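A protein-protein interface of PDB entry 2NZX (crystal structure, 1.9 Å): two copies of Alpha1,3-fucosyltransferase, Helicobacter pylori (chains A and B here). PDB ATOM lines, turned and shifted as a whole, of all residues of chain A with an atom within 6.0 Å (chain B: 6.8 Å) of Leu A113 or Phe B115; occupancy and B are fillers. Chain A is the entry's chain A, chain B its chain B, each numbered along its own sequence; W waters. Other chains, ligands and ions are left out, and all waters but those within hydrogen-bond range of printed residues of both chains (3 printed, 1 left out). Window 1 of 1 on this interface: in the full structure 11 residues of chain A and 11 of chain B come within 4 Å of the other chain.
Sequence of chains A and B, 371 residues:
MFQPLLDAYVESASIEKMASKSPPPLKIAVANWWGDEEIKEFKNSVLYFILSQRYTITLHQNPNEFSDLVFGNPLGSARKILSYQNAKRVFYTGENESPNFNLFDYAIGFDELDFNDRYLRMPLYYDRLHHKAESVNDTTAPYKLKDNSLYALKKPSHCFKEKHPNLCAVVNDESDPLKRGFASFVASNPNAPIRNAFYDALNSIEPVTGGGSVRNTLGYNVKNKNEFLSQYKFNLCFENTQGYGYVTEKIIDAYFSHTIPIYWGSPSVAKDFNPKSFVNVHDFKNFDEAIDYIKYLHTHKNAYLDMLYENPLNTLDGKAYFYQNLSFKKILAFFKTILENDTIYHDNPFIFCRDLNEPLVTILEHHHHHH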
ATOM      1  N   SER A  98      -4.317 -31.019 -12.340  1.00  0.00           N
ATOM      2  CA  SER A  98      -3.096 -30.632 -13.036  1.00  0.00           C
ATOM      3  C   SER A  98      -1.879 -30.807 -12.088  1.00  0.00           C
ATOM      4  O   SER A  98      -2.036 -30.734 -10.882  1.00  0.00           O
ATOM      5  CB  SER A  98      -3.221 -29.191 -13.503  1.00  0.00           C
ATOM      6  OG  SER A  98      -4.354 -29.101 -14.355  1.00  0.00           O
ATOM      7  N   PRO A  99      -0.666 -30.967 -12.638  1.00  0.00           N
ATOM      8  CA  PRO A  99       0.559 -31.180 -11.830  1.00  0.00           C
ATOM      9  C   PRO A  99       1.065 -29.983 -11.055  1.00  0.00           C
ATOM     10  O   PRO A  99       0.856 -28.877 -11.503  1.00  0.00           O
ATOM     11  CB  PRO A  99       1.591 -31.587 -12.869  1.00  0.00           C
ATOM     12  CG  PRO A  99       0.794 -31.784 -14.147  1.00  0.00           C
ATOM     13  CD  PRO A  99      -0.352 -30.894 -14.068  1.00  0.00           C
ATOM     14  N   PHE A 101       4.289 -28.410 -10.455  1.00  0.00           N
ATOM     15  CA  PHE A 101       5.666 -28.534 -10.886  1.00  0.00           C
ATOM     16  C   PHE A 101       6.695 -27.975  -9.877  1.00  0.00           C
ATOM     17  O   PHE A 101       7.896 -28.014 -10.134  1.00  0.00           O
ATOM     18  CB  PHE A 101       5.879 -27.885 -12.238  1.00  0.00           C
ATOM     19  CG  PHE A 101       5.169 -28.623 -13.363  1.00  0.00           C
ATOM     20  CD1 PHE A 101       5.674 -29.827 -13.866  1.00  0.00           C
ATOM     21  CD2 PHE A 101       4.014 -28.107 -13.922  1.00  0.00           C
ATOM     22  CE1 PHE A 101       5.035 -30.508 -14.944  1.00  0.00           C
ATOM     23  CE2 PHE A 101       3.348 -28.798 -14.994  1.00  0.00           C
ATOM     24  CZ  PHE A 101       3.861 -29.973 -15.495  1.00  0.00           C
ATOM     25  N   ASP A 111      -3.572 -32.883 -19.381  1.00  0.00           N
ATOM     26  CA  ASP A 111      -3.515 -31.501 -19.865  1.00  0.00           C
ATOM     27  C   ASP A 111      -2.843 -31.344 -21.211  1.00  0.00           C
ATOM     28  O   ASP A 111      -1.899 -32.035 -21.525  1.00  0.00           O
ATOM     29  CB  ASP A 111      -2.809 -30.570 -18.852  1.00  0.00           C
ATOM     30  CG  ASP A 111      -3.687 -30.261 -17.695  1.00  0.00           C
ATOM     31  OD1 ASP A 111      -4.811 -29.751 -17.936  1.00  0.00           O
ATOM     32  OD2 ASP A 111      -3.304 -30.562 -16.523  1.00  0.00           O
ATOM     33  N   GLU A 112      -3.353 -30.386 -21.985  1.00  0.00           N
ATOM     34  CA  GLU A 112      -2.832 -30.050 -23.306  1.00  0.00           C
ATOM     35  C   GLU A 112      -1.830 -28.935 -22.992  1.00  0.00           C
ATOM     36  O   GLU A 112      -2.116 -27.757 -23.169  1.00  0.00           O
ATOM     37  CB  GLU A 112      -3.971 -29.501 -24.168  1.00  0.00           C
ATOM     38  CG  GLU A 112      -5.066 -30.532 -24.410  1.00  0.00           C
ATOM     39  CD  GLU A 112      -6.183 -29.992 -25.310  1.00  0.00           C
ATOM     40  OE1 GLU A 112      -5.899 -29.761 -26.512  1.00  0.00           O
ATOM     41  OE2 GLU A 112      -7.302 -29.806 -24.796  1.00  0.00           O
ATOM     42  N   LEU A 113      -0.654 -29.303 -22.533  1.00  0.00           N
ATOM     43  CA  LEU A 113       0.361 -28.308 -22.124  1.00  0.00           C
ATOM     44  C   LEU A 113       1.685 -28.858 -22.600  1.00  0.00           C
ATOM     45  O   LEU A 113       1.840 -30.073 -22.752  1.00  0.00           O
ATOM     46  CB  LEU A 113       0.282 -28.251 -20.591  1.00  0.00           C
ATOM     47  CG  LEU A 113       1.312 -28.067 -19.501  1.00  0.00           C
ATOM     48  CD1 LEU A 113       0.534 -28.382 -18.220  1.00  0.00           C
ATOM     49  CD2 LEU A 113       2.494 -28.982 -19.628  1.00  0.00           C
ATOM     50  N   ASP A 114       2.643 -27.968 -22.855  1.00  0.00           N
ATOM     51  CA  ASP A 114       3.962 -28.361 -23.337  1.00  0.00           C
ATOM     52  C   ASP A 114       4.946 -27.705 -22.335  1.00  0.00           C
ATOM     53  O   ASP A 114       4.989 -26.468 -22.197  1.00  0.00           O
ATOM     54  CB  ASP A 114       4.130 -27.786 -24.750  1.00  0.00           C
ATOM     55  CG  ASP A 114       5.531 -27.848 -25.247  1.00  0.00           C
ATOM     56  OD1 ASP A 114       6.438 -28.399 -24.573  1.00  0.00           O
ATOM     57  OD2 ASP A 114       5.744 -27.323 -26.363  1.00  0.00           O
ATOM     58  N   PHE A 115       5.695 -28.531 -21.633  1.00  0.00           N
ATOM     59  CA  PHE A 115       6.669 -28.029 -20.633  1.00  0.00           C
ATOM     60  C   PHE A 115       7.984 -28.745 -21.005  1.00  0.00           C
ATOM     61  O   PHE A 115       8.739 -29.184 -20.172  1.00  0.00           O
ATOM     62  CB  PHE A 115       6.212 -28.372 -19.200  1.00  0.00           C
ATOM     63  CG  PHE A 115       6.844 -27.475 -18.121  1.00  0.00           C
ATOM     64  CD1 PHE A 115       7.805 -26.516 -18.481  1.00  0.00           C
ATOM     65  CD2 PHE A 115       6.406 -27.531 -16.783  1.00  0.00           C
ATOM     66  CE1 PHE A 115       8.309 -25.623 -17.571  1.00  0.00           C
ATOM     67  CE2 PHE A 115       6.930 -26.617 -15.820  1.00  0.00           C
ATOM     68  CZ  PHE A 115       7.885 -25.653 -16.238  1.00  0.00           C
ATOM     69  N   TYR A 119       6.918 -32.675 -19.123  1.00  0.00           N
ATOM     70  CA  TYR A 119       5.536 -33.146 -19.127  1.00  0.00           C
ATOM     71  C   TYR A 119       5.182 -34.036 -20.330  1.00  0.00           C
ATOM     72  O   TYR A 119       5.638 -33.836 -21.445  1.00  0.00           O
ATOM     73  CB  TYR A 119       4.595 -31.904 -19.104  1.00  0.00           C
ATOM     74  CG  TYR A 119       3.084 -32.207 -19.163  1.00  0.00           C
ATOM     75  CD1 TYR A 119       2.415 -32.708 -18.076  1.00  0.00           C
ATOM     76  CD2 TYR A 119       2.398 -32.122 -20.394  1.00  0.00           C
ATOM     77  CE1 TYR A 119       1.099 -33.142 -18.181  1.00  0.00           C
ATOM     78  CE2 TYR A 119       1.099 -32.571 -20.523  1.00  0.00           C
ATOM     79  CZ  TYR A 119       0.452 -33.081 -19.425  1.00  0.00           C
ATOM     80  OH  TYR A 119      -0.835 -33.575 -19.590  1.00  0.00           O
ATOM     81  N   ARG A 121       1.671 -35.956 -22.153  1.00  0.00           N
ATOM     82  CA  ARG A 121       0.203 -36.224 -22.076  1.00  0.00           C
ATOM     83  C   ARG A 121      -0.004 -37.721 -22.402  1.00  0.00           C
ATOM     84  O   ARG A 121       0.440 -38.167 -23.456  1.00  0.00           O
ATOM     85  CB  ARG A 121      -0.583 -35.401 -23.079  1.00  0.00           C
ATOM     86  CG  ARG A 121      -2.125 -35.764 -23.044  1.00  0.00           C
ATOM     87  CD  ARG A 121      -2.979 -34.713 -23.746  1.00  0.00           C
ATOM     88  NE  ARG A 121      -4.423 -34.964 -23.576  1.00  0.00           N
ATOM     89  CZ  ARG A 121      -5.209 -35.538 -24.509  1.00  0.00           C
ATOM     90  NH1 ARG A 121      -4.697 -35.938 -25.673  1.00  0.00           N
ATOM     91  NH2 ARG A 121      -6.502 -35.697 -24.281  1.00  0.00           N
ATOM     92  N   PHE B 101      -2.648 -24.724 -11.663  1.00  0.00           N
ATOM     93  CA  PHE B 101      -3.739 -24.545 -12.598  1.00  0.00           C
ATOM     94  C   PHE B 101      -5.041 -25.157 -12.180  1.00  0.00           C
ATOM     95  O   PHE B 101      -6.025 -25.091 -12.936  1.00  0.00           O
ATOM     96  CB  PHE B 101      -3.314 -25.076 -13.995  1.00  0.00           C
ATOM     97  CG  PHE B 101      -2.271 -24.218 -14.654  1.00  0.00           C
ATOM     98  CD1 PHE B 101      -2.622 -22.959 -15.178  1.00  0.00           C
ATOM     99  CD2 PHE B 101      -0.927 -24.634 -14.718  1.00  0.00           C
ATOM    100  CE1 PHE B 101      -1.643 -22.096 -15.755  1.00  0.00           C
ATOM    101  CE2 PHE B 101       0.032 -23.767 -15.296  1.00  0.00           C
ATOM    102  CZ  PHE B 101      -0.349 -22.499 -15.810  1.00  0.00           C
ATOM    103  N   ASP B 105      -7.423 -20.029 -13.258  1.00  0.00           N
ATOM    104  CA  ASP B 105      -7.802 -20.149 -14.637  1.00  0.00           C
ATOM    105  C   ASP B 105      -6.669 -19.689 -15.541  1.00  0.00           C
ATOM    106  O   ASP B 105      -6.411 -20.302 -16.576  1.00  0.00           O
ATOM    107  CB  ASP B 105      -9.064 -19.278 -14.864  1.00  0.00           C
ATOM    108  CG  ASP B 105     -10.188 -19.701 -13.947  1.00  0.00           C
ATOM    109  OD1 ASP B 105     -10.470 -19.023 -12.922  1.00  0.00           O
ATOM    110  OD2 ASP B 105     -10.768 -20.758 -14.278  1.00  0.00           O
ATOM    111  N   LEU B 113       6.836 -22.437 -20.294  1.00  0.00           N
ATOM    112  CA  LEU B 113       5.796 -23.398 -20.499  1.00  0.00           C
ATOM    113  C   LEU B 113       4.794 -22.815 -21.449  1.00  0.00           C
ATOM    114  O   LEU B 113       4.679 -21.610 -21.554  1.00  0.00           O
ATOM    115  CB  LEU B 113       5.253 -23.657 -19.094  1.00  0.00           C
ATOM    116  CG  LEU B 113       3.918 -24.094 -18.575  1.00  0.00           C
ATOM    117  CD1 LEU B 113       4.046 -23.980 -17.051  1.00  0.00           C
ATOM    118  CD2 LEU B 113       2.847 -23.218 -19.074  1.00  0.00           C
ATOM    119  N   ASP B 114       4.084 -23.697 -22.145  1.00  0.00           N
ATOM    120  CA  ASP B 114       3.075 -23.271 -23.107  1.00  0.00           C
ATOM    121  C   ASP B 114       1.817 -23.999 -22.722  1.00  0.00           C
ATOM    122  O   ASP B 114       1.765 -25.261 -22.734  1.00  0.00           O
ATOM    123  CB  ASP B 114       3.528 -23.642 -24.520  1.00  0.00           C
ATOM    124  CG  ASP B 114       2.495 -23.307 -25.601  1.00  0.00           C
ATOM    125  OD1 ASP B 114       1.412 -22.794 -25.274  1.00  0.00           O
ATOM    126  OD2 ASP B 114       2.785 -23.595 -26.783  1.00  0.00           O
ATOM    127  N   PHE B 115       0.808 -23.243 -22.341  1.00  0.00           N
ATOM    128  CA  PHE B 115      -0.455 -23.864 -21.983  1.00  0.00           C
ATOM    129  C   PHE B 115      -1.521 -23.083 -22.776  1.00  0.00           C
ATOM    130  O   PHE B 115      -2.608 -22.771 -22.259  1.00  0.00           O
ATOM    131  CB  PHE B 115      -0.658 -23.762 -20.468  1.00  0.00           C
ATOM    132  CG  PHE B 115      -1.649 -24.753 -19.898  1.00  0.00           C
ATOM    133  CD1 PHE B 115      -2.425 -25.614 -20.727  1.00  0.00           C
ATOM    134  CD2 PHE B 115      -1.861 -24.797 -18.511  1.00  0.00           C
ATOM    135  CE1 PHE B 115      -3.366 -26.465 -20.136  1.00  0.00           C
ATOM    136  CE2 PHE B 115      -2.784 -25.634 -17.953  1.00  0.00           C
ATOM    137  CZ  PHE B 115      -3.539 -26.464 -18.753  1.00  0.00           C
ATOM    138  N   ASN B 116      -1.175 -22.772 -24.027  1.00  0.00           N
ATOM    139  CA  ASN B 116      -2.031 -22.006 -24.940  1.00  0.00           C
ATOM    140  C   ASN B 116      -2.525 -20.729 -24.293  1.00  0.00           C
ATOM    141  O   ASN B 116      -1.700 -19.930 -23.846  1.00  0.00           O
ATOM    142  CB  ASN B 116      -3.161 -22.887 -25.441  1.00  0.00           C
ATOM    143  CG  ASN B 116      -2.635 -23.930 -26.381  1.00  0.00           C
ATOM    144  OD1 ASN B 116      -2.015 -23.585 -27.424  1.00  0.00           O
ATOM    145  ND2 ASN B 116      -2.819 -25.220 -26.029  1.00  0.00           N
ATOM    146  N   ASP B 117      -3.824 -20.498 -24.264  1.00  0.00           N
ATOM    147  CA  ASP B 117      -4.329 -19.271 -23.667  1.00  0.00           C
ATOM    148  C   ASP B 117      -4.299 -19.139 -22.171  1.00  0.00           C
ATOM    149  O   ASP B 117      -4.562 -18.058 -21.657  1.00  0.00           O
ATOM    150  CB  ASP B 117      -5.756 -18.993 -24.172  1.00  0.00           C
ATOM    151  CG  ASP B 117      -5.772 -18.747 -25.685  1.00  0.00           C
ATOM    152  OD1 ASP B 117      -4.907 -17.982 -26.197  1.00  0.00           O
ATOM    153  OD2 ASP B 117      -6.624 -19.344 -26.364  1.00  0.00           O
ATOM    154  N   ARG B 118      -3.949 -20.204 -21.439  1.00  0.00           N
ATOM    155  CA  ARG B 118      -3.961 -20.113 -19.979  1.00  0.00           C
ATOM    156  C   ARG B 118      -2.721 -19.544 -19.283  1.00  0.00           C
ATOM    157  O   ARG B 118      -2.752 -19.208 -18.065  1.00  0.00           O
ATOM    158  CB  ARG B 118      -4.256 -21.495 -19.367  1.00  0.00           C
ATOM    159  CG  ARG B 118      -5.701 -21.970 -19.726  1.00  0.00           C
ATOM    160  CD  ARG B 118      -6.052 -23.275 -19.051  1.00  0.00           C
ATOM    161  NE  ARG B 118      -6.145 -23.019 -17.622  1.00  0.00           N
ATOM    162  CZ  ARG B 118      -6.206 -23.974 -16.689  1.00  0.00           C
ATOM    163  NH1 ARG B 118      -6.195 -25.268 -17.025  1.00  0.00           N
ATOM    164  NH2 ARG B 118      -6.315 -23.627 -15.415  1.00  0.00           N
ATOM    165  N   TYR B 119      -1.642 -19.413 -20.048  1.00  0.00           N
ATOM    166  CA  TYR B 119      -0.392 -18.987 -19.435  1.00  0.00           C
ATOM    167  C   TYR B 119       0.398 -17.983 -20.233  1.00  0.00           C
ATOM    168  O   TYR B 119       0.524 -18.164 -21.420  1.00  0.00           O
ATOM    169  CB  TYR B 119       0.469 -20.216 -19.227  1.00  0.00           C
ATOM    170  CG  TYR B 119       1.834 -19.919 -18.623  1.00  0.00           C
ATOM    171  CD1 TYR B 119       1.949 -19.567 -17.286  1.00  0.00           C
ATOM    172  CD2 TYR B 119       2.986 -19.879 -19.415  1.00  0.00           C
ATOM    173  CE1 TYR B 119       3.198 -19.145 -16.724  1.00  0.00           C
ATOM    174  CE2 TYR B 119       4.234 -19.455 -18.872  1.00  0.00           C
ATOM    175  CZ  TYR B 119       4.313 -19.084 -17.532  1.00  0.00           C
ATOM    176  OH  TYR B 119       5.511 -18.544 -17.049  1.00  0.00           O
ATOM    177  N   TYR B 345     -11.955 -22.627 -15.930  1.00  0.00           N
ATOM    178  CA  TYR B 345     -11.090 -23.810 -15.877  1.00  0.00           C
ATOM    179  C   TYR B 345     -10.802 -24.248 -14.477  1.00  0.00           C
ATOM    180  O   TYR B 345     -10.400 -25.398 -14.265  1.00  0.00           O
ATOM    181  CB  TYR B 345      -9.748 -23.516 -16.476  1.00  0.00           C
ATOM    182  CG  TYR B 345      -9.751 -23.044 -17.873  1.00  0.00           C
ATOM    183  CD1 TYR B 345      -9.718 -21.683 -18.184  1.00  0.00           C
ATOM    184  CD2 TYR B 345      -9.779 -23.961 -18.905  1.00  0.00           C
ATOM    185  CE1 TYR B 345      -9.705 -21.267 -19.527  1.00  0.00           C
ATOM    186  CE2 TYR B 345      -9.784 -23.559 -20.214  1.00  0.00           C
ATOM    187  CZ  TYR B 345      -9.739 -22.225 -20.524  1.00  0.00           C
ATOM    188  OH  TYR B 345      -9.670 -21.925 -21.852  1.00  0.00           O
HETATM  189  O   HOH W   1      -1.205 -27.107 -11.598  1.00  0.00           O
HETATM  190  O   HOH W   2      -6.139 -27.358 -14.843  1.00  0.00           O
HETATM  191  O   HOH W   3      -4.224 -25.880 -23.917  1.00  0.00           O
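Among the printed residues, pairs that only touch across the chains: Glu A112 with Phe B115, Leu A113 with Asp B114, Asp A114 with Leu B113, Asp A111 with Phe B115, Leu A113 with Phe B115, Phe A115 with Leu B113 and Glu A112 with Asn B116.
Of chain B, only Asp B114 and Phe B115 come within 4 Å of Leu A113.
Of the printed residues of chain A, Asn B116 touches Glu A112 (3.9 Å).
Of the printed residues of chain B, Glu A112 touches Phe B115 (3.3 Å) and Asn B116 (3.9 Å).
Printed residues of chain A within 4 Å of Leu B113: Asp A114 (3.6 Å) and Phe A115 (3.9 Å).
Of the printed residues of chain B, Phe A115 touches Leu B113.
Printed residues of chain B within 4 Å of Asp A114: Leu B113 (3.6 Å) and Asp B114 (2.8 Å).
Phe A101 touches none of the printed residues of chain B.
Tyr B119 touches none of the printed residues of chain A.
Water W2 lies within hydrogen-bond range of the side-chain hydroxyl (OG) of Ser A98 (2.5 Å), the backbone carbonyl oxygen (O) of Phe B101 (3.0 Å) and the guanidinium group (NH1) of Arg B118 (3.0 Å).
Water W3 lies within hydrogen-bond range of ND2 of Asn B116 (2.6 Å) and O of Glu A112 (2.9 Å).
Water W1 lies within hydrogen-bond range of the backbone carbonyl oxygen of Pro A99 and the backbone NH of Phe B101.
Of the 10 printed residues of chain A, 5 touch a printed residue of chain B.
Printed residues of chain A that touch a printed residue of chain B: Asp A111, Glu A112, Leu A113, Asp A114 and Phe A115.
Along chain A the printed residues that touch a printed residue of chain B span positions 111 to 115.
Of the 10 printed residues of chain B, 4 touch a printed residue of chain A.
Leu A113 touches Asp B114, and with the chains exchanged Asp A114 touches Leu B113.
Leu A113 touches Phe B115, and with the chains exchanged Phe A115 touches Leu B113.
Asp B114 touches its own counterpart, Asp A114.
Of the 8 pairs that touch across the chains among the printed residues, 5 have their exchanged pair printed and touching as well.
OG of Ser A98 lies within hydrogen-bond range of OD2 of Asp A111 (2.8 Å).
O of Asp A111 is in hydrogen-bond range of OH of Tyr A119 (2.7 Å).
The side-chain carboxylate (OD1) of Asp B114 is in hydrogen-bond range of the backbone NH (N) of Asn B116, 2.9 Å away.
The backbone NH of Asp A114 sits at hydrogen-bond distance from the backbone carbonyl oxygen of Asp B114.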
